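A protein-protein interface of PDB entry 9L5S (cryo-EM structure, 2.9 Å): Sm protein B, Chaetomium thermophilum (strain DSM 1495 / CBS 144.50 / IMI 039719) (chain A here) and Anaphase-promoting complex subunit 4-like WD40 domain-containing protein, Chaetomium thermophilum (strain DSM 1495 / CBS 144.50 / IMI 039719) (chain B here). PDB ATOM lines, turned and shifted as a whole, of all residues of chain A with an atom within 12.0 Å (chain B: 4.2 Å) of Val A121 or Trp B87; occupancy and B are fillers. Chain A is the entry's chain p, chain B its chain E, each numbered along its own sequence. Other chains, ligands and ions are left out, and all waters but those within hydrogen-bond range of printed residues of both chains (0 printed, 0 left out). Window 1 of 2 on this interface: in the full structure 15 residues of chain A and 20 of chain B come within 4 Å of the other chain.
O of Tyr B96 touches CD2 of Leu A115 (3.7 Å). Ala A117 touches Tyr B96 (CA to O, 3.8 Å). Asn B95 touches Gly A118 (OD1 to CA, 3.4 Å). Pro A119 touches Asn B95. Gly A120 touches Ser B57 (CA to O, 3.3 Å). Gly A120 touches Met B85. Gly A120 touches Trp B87 (CA to CH2, 3.98 Å). CA of Leu B56 touches O of Val A121, at 3.98 Å. Val A121 touches Trp B87. Leu B56 touches Ala A122.
The backbone carbonyl oxygen of Leu B86 lies within hydrogen-bond range of the backbone NH of Tyr B96 (2.8 Å). The backbone carbonyl oxygen (O) of Leu B86 is in hydrogen-bond range of the side-chain amide nitrogen (ND2) of Asn B95 (2.7 Å). The backbone NH (N) of Trp B87 sits at hydrogen-bond distance from the backbone carbonyl oxygen (O) of Ile B75, 2.9 Å away. The backbone carbonyl oxygen of Ser B77 sits at hydrogen-bond distance from the backbone NH of Met B85. OG of Ser B77 lies within hydrogen-bond range of NE1 of Trp B87, at 3.4 Å. The backbone carbonyl oxygen (O) of Met B346 sits at hydrogen-bond distance from the backbone NH (N) of Leu B56 (2.8 Å).
Hydrophobic or aromatic side chains of chain B within 4 Å of the printed part of chain A: Leu B56, Met B85, Trp B87 and Tyr B96. Along chain B the printed residues that touch a printed residue of chain A span positions 56 to 96. Among the printed residues, 13 pairs touch across the chains.
O of Thr A116 sits close to O of Tyr B96, 3.0 Å away. N of Gly A120 sits at hydrogen-bond distance from OD1 of Asn B95, at 3.3 Å. O of Ser B57 is in hydrogen-bond range of N of Val A121 (3.2 Å).
Of the printed residues of chain B, Leu A115 touches Tyr B96 (3.7 Å). Of chain B, only Leu B56 (3.98 Å), Ser B57 (3.2 Å) and Trp B87 (3.8 Å) come within 4 Å of Val A121. Of the printed residues of chain B, Ala A122 touches Leu B56. Ser B57 touches two residues of chain A. No residue of chain A comes within 4 Å of Ser B77. No residue of chain A comes within 4 Å of Leu B86. Trp B87 touches just these residues of chain A: Gly A120 (3.98 Å) and Val A121 (3.8 Å). No residue of chain A comes within 4 Å of Arg B88. No residue of chain A comes within 4 Å of Val B89. Of chain A, only Gly A118, Pro A119 and Gly A120 come within 4 Å of Asn B95. Of chain A, only Leu A115 (3.7 Å), Thr A116 (3.0 Å) and Ala A117 (3.8 Å) come within 4 Å of Tyr B96. The nearest printed residue of chain B that does not touch Leu A115 is Leu B86 (4.3 Å).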
ATOM      1  N   LEU A 115      26.335   1.779   5.042  1.00  0.00           N
ATOM      2  CA  LEU A 115      26.449   0.502   5.741  1.00  0.00           C
ATOM      3  C   LEU A 115      25.635   0.551   7.027  1.00  0.00           C
ATOM      4  O   LEU A 115      26.035   1.193   8.004  1.00  0.00           O
ATOM      5  CB  LEU A 115      27.912   0.188   6.039  1.00  0.00           C
ATOM      6  CG  LEU A 115      28.173  -1.096   6.833  1.00  0.00           C
ATOM      7  CD1 LEU A 115      28.027  -2.334   5.966  1.00  0.00           C
ATOM      8  CD2 LEU A 115      29.547  -1.055   7.486  1.00  0.00           C
ATOM      9  N   THR A 116      24.490  -0.126   7.030  1.00  0.00           N
ATOM     10  CA  THR A 116      23.642  -0.161   8.211  1.00  0.00           C
ATOM     11  C   THR A 116      24.163  -1.182   9.219  1.00  0.00           C
ATOM     12  O   THR A 116      24.994  -2.040   8.910  1.00  0.00           O
ATOM     13  CB  THR A 116      22.201  -0.496   7.830  1.00  0.00           C
ATOM     14  OG1 THR A 116      21.393  -0.551   9.012  1.00  0.00           O
ATOM     15  CG2 THR A 116      22.137  -1.840   7.116  1.00  0.00           C
ATOM     16  N   ALA A 117      23.654  -1.079  10.443  1.00  0.00           N
ATOM     17  CA  ALA A 117      24.000  -2.025  11.492  1.00  0.00           C
ATOM     18  C   ALA A 117      23.227  -3.325  11.310  1.00  0.00           C
ATOM     19  O   ALA A 117      22.264  -3.399  10.540  1.00  0.00           O
ATOM     20  CB  ALA A 117      23.714  -1.432  12.870  1.00  0.00           C
ATOM     21  N   GLY A 118      23.657  -4.356  12.029  1.00  0.00           N
ATOM     22  CA  GLY A 118      23.046  -5.657  11.914  1.00  0.00           C
ATOM     23  C   GLY A 118      22.085  -5.973  13.040  1.00  0.00           C
ATOM     24  O   GLY A 118      21.953  -5.220  14.010  1.00  0.00           O
ATOM     25  N   PRO A 119      21.392  -7.105  12.930  1.00  0.00           N
ATOM     26  CA  PRO A 119      20.470  -7.537  13.986  1.00  0.00           C
ATOM     27  C   PRO A 119      21.076  -8.474  15.018  1.00  0.00           C
ATOM     28  O   PRO A 119      20.335  -8.989  15.862  1.00  0.00           O
ATOM     29  CB  PRO A 119      19.389  -8.258  13.175  1.00  0.00           C
ATOM     30  CG  PRO A 119      20.178  -8.941  12.096  1.00  0.00           C
ATOM     31  CD  PRO A 119      21.347  -8.019  11.774  1.00  0.00           C
ATOM     32  N   GLY A 120      22.388  -8.710  14.978  1.00  0.00           N
ATOM     33  CA  GLY A 120      22.993  -9.640  15.902  1.00  0.00           C
ATOM     34  C   GLY A 120      23.266  -9.026  17.260  1.00  0.00           C
ATOM     35  O   GLY A 120      23.314  -7.809  17.435  1.00  0.00           O
ATOM     36  N   VAL A 121      23.446  -9.904  18.246  1.00  0.00           N
ATOM     37  CA  VAL A 121      23.749  -9.504  19.611  1.00  0.00           C
ATOM     38  C   VAL A 121      24.926 -10.326  20.111  1.00  0.00           C
ATOM     39  O   VAL A 121      25.251 -11.387  19.575  1.00  0.00           O
ATOM     40  CB  VAL A 121      22.545  -9.663  20.569  1.00  0.00           C
ATOM     41  CG1 VAL A 121      21.409  -8.727  20.175  1.00  0.00           C
ATOM     42  CG2 VAL A 121      22.071 -11.107  20.598  1.00  0.00           C
ATOM     43  N   ALA A 122      25.568  -9.809  21.151  1.00  0.00           N
ATOM     44  CA  ALA A 122      26.725 -10.445  21.757  1.00  0.00           C
ATOM     45  C   ALA A 122      26.565 -10.438  23.268  1.00  0.00           C
ATOM     46  O   ALA A 122      26.191  -9.420  23.857  1.00  0.00           O
ATOM     47  CB  ALA A 122      28.015  -9.729  21.351  1.00  0.00           C
ATOM     48  N   ARG A 123      26.846 -11.577  23.891  1.00  0.00           N
ATOM     49  CA  ARG A 123      26.730 -11.735  25.330  1.00  0.00           C
ATOM     50  C   ARG A 123      27.822 -12.673  25.819  1.00  0.00           C
ATOM     51  O   ARG A 123      28.302 -13.520  25.056  1.00  0.00           O
ATOM     52  CB  ARG A 123      25.346 -12.278  25.725  1.00  0.00           C
ATOM     53  CG  ARG A 123      25.048 -13.685  25.231  1.00  0.00           C
ATOM     54  CD  ARG A 123      23.937 -14.338  26.039  1.00  0.00           C
ATOM     55  NE  ARG A 123      23.686 -15.711  25.616  1.00  0.00           N
ATOM     56  CZ  ARG A 123      24.381 -16.763  26.025  1.00  0.00           C
ATOM     57  NH1 ARG A 123      25.372 -16.642  26.892  1.00  0.00           N
ATOM     58  NH2 ARG A 123      24.071 -17.968  25.555  1.00  0.00           N
ATOM     59  N   PRO A 124      28.258 -12.525  27.071  1.00  0.00           N
ATOM     60  CA  PRO A 124      29.226 -13.475  27.628  1.00  0.00           C
ATOM     61  C   PRO A 124      28.629 -14.865  27.778  1.00  0.00           C
ATOM     62  O   PRO A 124      27.425 -15.034  27.979  1.00  0.00           O
ATOM     63  CB  PRO A 124      29.576 -12.871  28.993  1.00  0.00           C
ATOM     64  CG  PRO A 124      29.245 -11.424  28.861  1.00  0.00           C
ATOM     65  CD  PRO A 124      28.060 -11.362  27.953  1.00  0.00           C
ATOM     66  N   ALA A 125      29.496 -15.867  27.678  1.00  0.00           N
ATOM     67  CA  ALA A 125      29.063 -17.257  27.730  1.00  0.00           C
ATOM     68  C   ALA A 125      30.223 -18.113  28.214  1.00  0.00           C
ATOM     69  O   ALA A 125      31.372 -17.671  28.265  1.00  0.00           O
ATOM     70  CB  ALA A 125      28.563 -17.737  26.365  1.00  0.00           C
ATOM     71  N   LEU B  56      28.561 -14.886  19.742  1.00  0.00           N
ATOM     72  CA  LEU B  56      28.076 -14.037  18.662  1.00  0.00           C
ATOM     73  C   LEU B  56      26.992 -14.816  17.934  1.00  0.00           C
ATOM     74  O   LEU B  56      27.257 -15.901  17.401  1.00  0.00           O
ATOM     75  CB  LEU B  56      29.199 -13.644  17.699  1.00  0.00           C
ATOM     76  CG  LEU B  56      30.453 -13.000  18.290  1.00  0.00           C
ATOM     77  CD1 LEU B  56      31.596 -13.059  17.294  1.00  0.00           C
ATOM     78  CD2 LEU B  56      30.179 -11.569  18.708  1.00  0.00           C
ATOM     79  N   SER B  57      25.778 -14.273  17.929  1.00  0.00           N
ATOM     80  CA  SER B  57      24.628 -14.945  17.347  1.00  0.00           C
ATOM     81  C   SER B  57      23.771 -13.928  16.611  1.00  0.00           C
ATOM     82  O   SER B  57      23.863 -12.721  16.842  1.00  0.00           O
ATOM     83  CB  SER B  57      23.792 -15.663  18.413  1.00  0.00           C
ATOM     84  OG  SER B  57      23.528 -14.808  19.510  1.00  0.00           O
ATOM     85  N   LEU B  74      38.121  -7.055  13.125  1.00  0.00           N
ATOM     86  CA  LEU B  74      36.821  -7.250  12.498  1.00  0.00           C
ATOM     87  C   LEU B  74      36.641  -8.720  12.155  1.00  0.00           C
ATOM     88  O   LEU B  74      37.594  -9.383  11.734  1.00  0.00           O
ATOM     89  CB  LEU B  74      36.686  -6.390  11.233  1.00  0.00           C
ATOM     90  CG  LEU B  74      37.153  -4.934  11.321  1.00  0.00           C
ATOM     91  CD1 LEU B  74      37.134  -4.260   9.957  1.00  0.00           C
ATOM     92  CD2 LEU B  74      36.295  -4.163  12.309  1.00  0.00           C
ATOM     93  N   ILE B  75      35.423  -9.227  12.338  1.00  0.00           N
ATOM     94  CA  ILE B  75      35.060 -10.594  11.978  1.00  0.00           C
ATOM     95  C   ILE B  75      33.982 -10.536  10.905  1.00  0.00           C
ATOM     96  O   ILE B  75      33.030  -9.757  11.016  1.00  0.00           O
ATOM     97  CB  ILE B  75      34.581 -11.394  13.204  1.00  0.00           C
ATOM     98  CG1 ILE B  75      35.709 -11.532  14.220  1.00  0.00           C
ATOM     99  CG2 ILE B  75      34.059 -12.767  12.807  1.00  0.00           C
ATOM    100  CD1 ILE B  75      35.311 -12.270  15.474  1.00  0.00           C
ATOM    101  N   SER B  77      31.411 -13.166   8.804  1.00  0.00           N
ATOM    102  CA  SER B  77      30.884 -14.526   8.803  1.00  0.00           C
ATOM    103  C   SER B  77      29.796 -14.659   7.747  1.00  0.00           C
ATOM    104  O   SER B  77      28.882 -13.832   7.684  1.00  0.00           O
ATOM    105  CB  SER B  77      30.338 -14.902  10.181  1.00  0.00           C
ATOM    106  OG  SER B  77      29.234 -14.088  10.533  1.00  0.00           O
ATOM    107  N   MET B  85      27.525 -11.306   8.067  1.00  0.00           N
ATOM    108  CA  MET B  85      27.478 -10.457   9.249  1.00  0.00           C
ATOM    109  C   MET B  85      28.893 -10.025   9.616  1.00  0.00           C
ATOM    110  O   MET B  85      29.806 -10.856   9.697  1.00  0.00           O
ATOM    111  CB  MET B  85      26.791 -11.182  10.409  1.00  0.00           C
ATOM    112  CG  MET B  85      25.298 -11.393  10.151  1.00  0.00           C
ATOM    113  SD  MET B  85      24.425 -12.499  11.279  1.00  0.00           S
ATOM    114  CE  MET B  85      24.043 -11.412  12.640  1.00  0.00           C
ATOM    115  N   LEU B  86      29.065  -8.717   9.805  1.00  0.00           N
ATOM    116  CA  LEU B  86      30.341  -8.083  10.108  1.00  0.00           C
ATOM    117  C   LEU B  86      30.287  -7.548  11.531  1.00  0.00           C
ATOM    118  O   LEU B  86      29.478  -6.655  11.826  1.00  0.00           O
ATOM    119  CB  LEU B  86      30.632  -6.943   9.132  1.00  0.00           C
ATOM    120  CG  LEU B  86      30.486  -7.205   7.634  1.00  0.00           C
ATOM    121  CD1 LEU B  86      30.255  -5.903   6.889  1.00  0.00           C
ATOM    122  CD2 LEU B  86      31.718  -7.894   7.105  1.00  0.00           C
ATOM    123  N   TRP B  87      31.174  -8.067  12.381  1.00  0.00           N
ATOM    124  CA  TRP B  87      31.223  -7.809  13.811  1.00  0.00           C
ATOM    125  C   TRP B  87      32.527  -7.109  14.167  1.00  0.00           C
ATOM    126  O   TRP B  87      33.558  -7.316  13.519  1.00  0.00           O
ATOM    127  CB  TRP B  87      31.148  -9.110  14.626  1.00  0.00           C
ATOM    128  CG  TRP B  87      30.142 -10.114  14.161  1.00  0.00           C
ATOM    129  CD1 TRP B  87      30.233 -10.927  13.067  1.00  0.00           C
ATOM    130  CD2 TRP B  87      28.914 -10.453  14.809  1.00  0.00           C
ATOM    131  NE1 TRP B  87      29.123 -11.725  12.978  1.00  0.00           N
ATOM    132  CE2 TRP B  87      28.300 -11.458  14.038  1.00  0.00           C
ATOM    133  CE3 TRP B  87      28.267  -9.994  15.960  1.00  0.00           C
ATOM    134  CZ2 TRP B  87      27.076 -12.014  14.382  1.00  0.00           C
ATOM    135  CZ3 TRP B  87      27.049 -10.546  16.297  1.00  0.00           C
ATOM    136  CH2 TRP B  87      26.466 -11.544  15.511  1.00  0.00           C
ATOM    137  N   ARG B  88      32.479  -6.303  15.225  1.00  0.00           N
ATOM    138  CA  ARG B  88      33.657  -5.646  15.775  1.00  0.00           C
ATOM    139  C   ARG B  88      34.085  -6.381  17.040  1.00  0.00           C
ATOM    140  O   ARG B  88      33.278  -6.565  17.956  1.00  0.00           O
ATOM    141  CB  ARG B  88      33.362  -4.178  16.084  1.00  0.00           C
ATOM    142  CG  ARG B  88      34.536  -3.240  15.875  1.00  0.00           C
ATOM    143  CD  ARG B  88      34.054  -1.813  15.673  1.00  0.00           C
ATOM    144  NE  ARG B  88      33.793  -1.514  14.271  1.00  0.00           N
ATOM    145  CZ  ARG B  88      32.839  -0.697  13.845  1.00  0.00           C
ATOM    146  NH1 ARG B  88      32.029  -0.082  14.690  1.00  0.00           N
ATOM    147  NH2 ARG B  88      32.694  -0.493  12.539  1.00  0.00           N
ATOM    148  N   VAL B  89      35.350  -6.801  17.087  1.00  0.00           N
ATOM    149  CA  VAL B  89      35.818  -7.634  18.191  1.00  0.00           C
ATOM    150  C   VAL B  89      36.042  -6.804  19.447  1.00  0.00           C
ATOM    151  O   VAL B  89      35.576  -7.158  20.536  1.00  0.00           O
ATOM    152  CB  VAL B  89      37.103  -8.383  17.792  1.00  0.00           C
ATOM    153  CG1 VAL B  89      37.401  -9.491  18.790  1.00  0.00           C
ATOM    154  CG2 VAL B  89      36.982  -8.937  16.397  1.00  0.00           C
ATOM    155  N   GLU B  94      30.085  -5.263  18.802  1.00  0.00           N
ATOM    156  CA  GLU B  94      28.899  -4.784  18.112  1.00  0.00           C
ATOM    157  C   GLU B  94      28.860  -5.338  16.696  1.00  0.00           C
ATOM    158  O   GLU B  94      29.870  -5.307  15.984  1.00  0.00           O
ATOM    159  CB  GLU B  94      28.882  -3.252  18.082  1.00  0.00           C
ATOM    160  CG  GLU B  94      27.725  -2.640  17.314  1.00  0.00           C
ATOM    161  CD  GLU B  94      26.532  -2.339  18.198  1.00  0.00           C
ATOM    162  OE1 GLU B  94      26.737  -2.028  19.391  1.00  0.00           O
ATOM    163  OE2 GLU B  94      25.391  -2.408  17.698  1.00  0.00           O
ATOM    164  N   ASN B  95      27.701  -5.857  16.301  1.00  0.00           N
ATOM    165  CA  ASN B  95      27.443  -6.144  14.898  1.00  0.00           C
ATOM    166  C   ASN B  95      27.279  -4.828  14.152  1.00  0.00           C
ATOM    167  O   ASN B  95      26.397  -4.027  14.477  1.00  0.00           O
ATOM    168  CB  ASN B  95      26.182  -6.997  14.759  1.00  0.00           C
ATOM    169  CG  ASN B  95      25.962  -7.512  13.343  1.00  0.00           C
ATOM    170  OD1 ASN B  95      25.007  -8.233  13.059  1.00  0.00           O
ATOM    171  ND2 ASN B  95      26.876  -7.164  12.453  1.00  0.00           N
ATOM    172  N   TYR B  96      28.122  -4.599  13.146  1.00  0.00           N
ATOM    173  CA  TYR B  96      28.073  -3.345  12.412  1.00  0.00           C
ATOM    174  C   TYR B  96      27.755  -3.493  10.933  1.00  0.00           C
ATOM    175  O   TYR B  96      27.581  -2.469  10.265  1.00  0.00           O
ATOM    176  CB  TYR B  96      29.397  -2.571  12.562  1.00  0.00           C
ATOM    177  CG  TYR B  96      30.588  -3.170  11.843  1.00  0.00           C
ATOM    178  CD1 TYR B  96      31.362  -4.157  12.437  1.00  0.00           C
ATOM    179  CD2 TYR B  96      30.965  -2.716  10.581  1.00  0.00           C
ATOM    180  CE1 TYR B  96      32.456  -4.697  11.783  1.00  0.00           C
ATOM    181  CE2 TYR B  96      32.054  -3.250   9.923  1.00  0.00           C
ATOM    182  CZ  TYR B  96      32.796  -4.239  10.528  1.00  0.00           C
ATOM    183  OH  TYR B  96      33.883  -4.770   9.876  1.00  0.00           O
ATOM    184  N   MET B 346      28.859 -18.335  16.935  1.00  0.00           N
ATOM    185  CA  MET B 346      30.308 -18.241  17.041  1.00  0.00           C
ATOM    186  C   MET B 346      30.702 -18.001  18.490  1.00  0.00           C
ATOM    187  O   MET B 346      30.022 -17.273  19.216  1.00  0.00           O
ATOM    188  CB  MET B 346      30.866 -17.119  16.164  1.00  0.00           C
ATOM    189  CG  MET B 346      30.705 -17.354  14.681  1.00  0.00           C
ATOM    190  SD  MET B 346      31.441 -16.027  13.716  1.00  0.00           S
ATOM    191  CE  MET B 346      30.236 -14.735  13.980  1.00  0.00           C
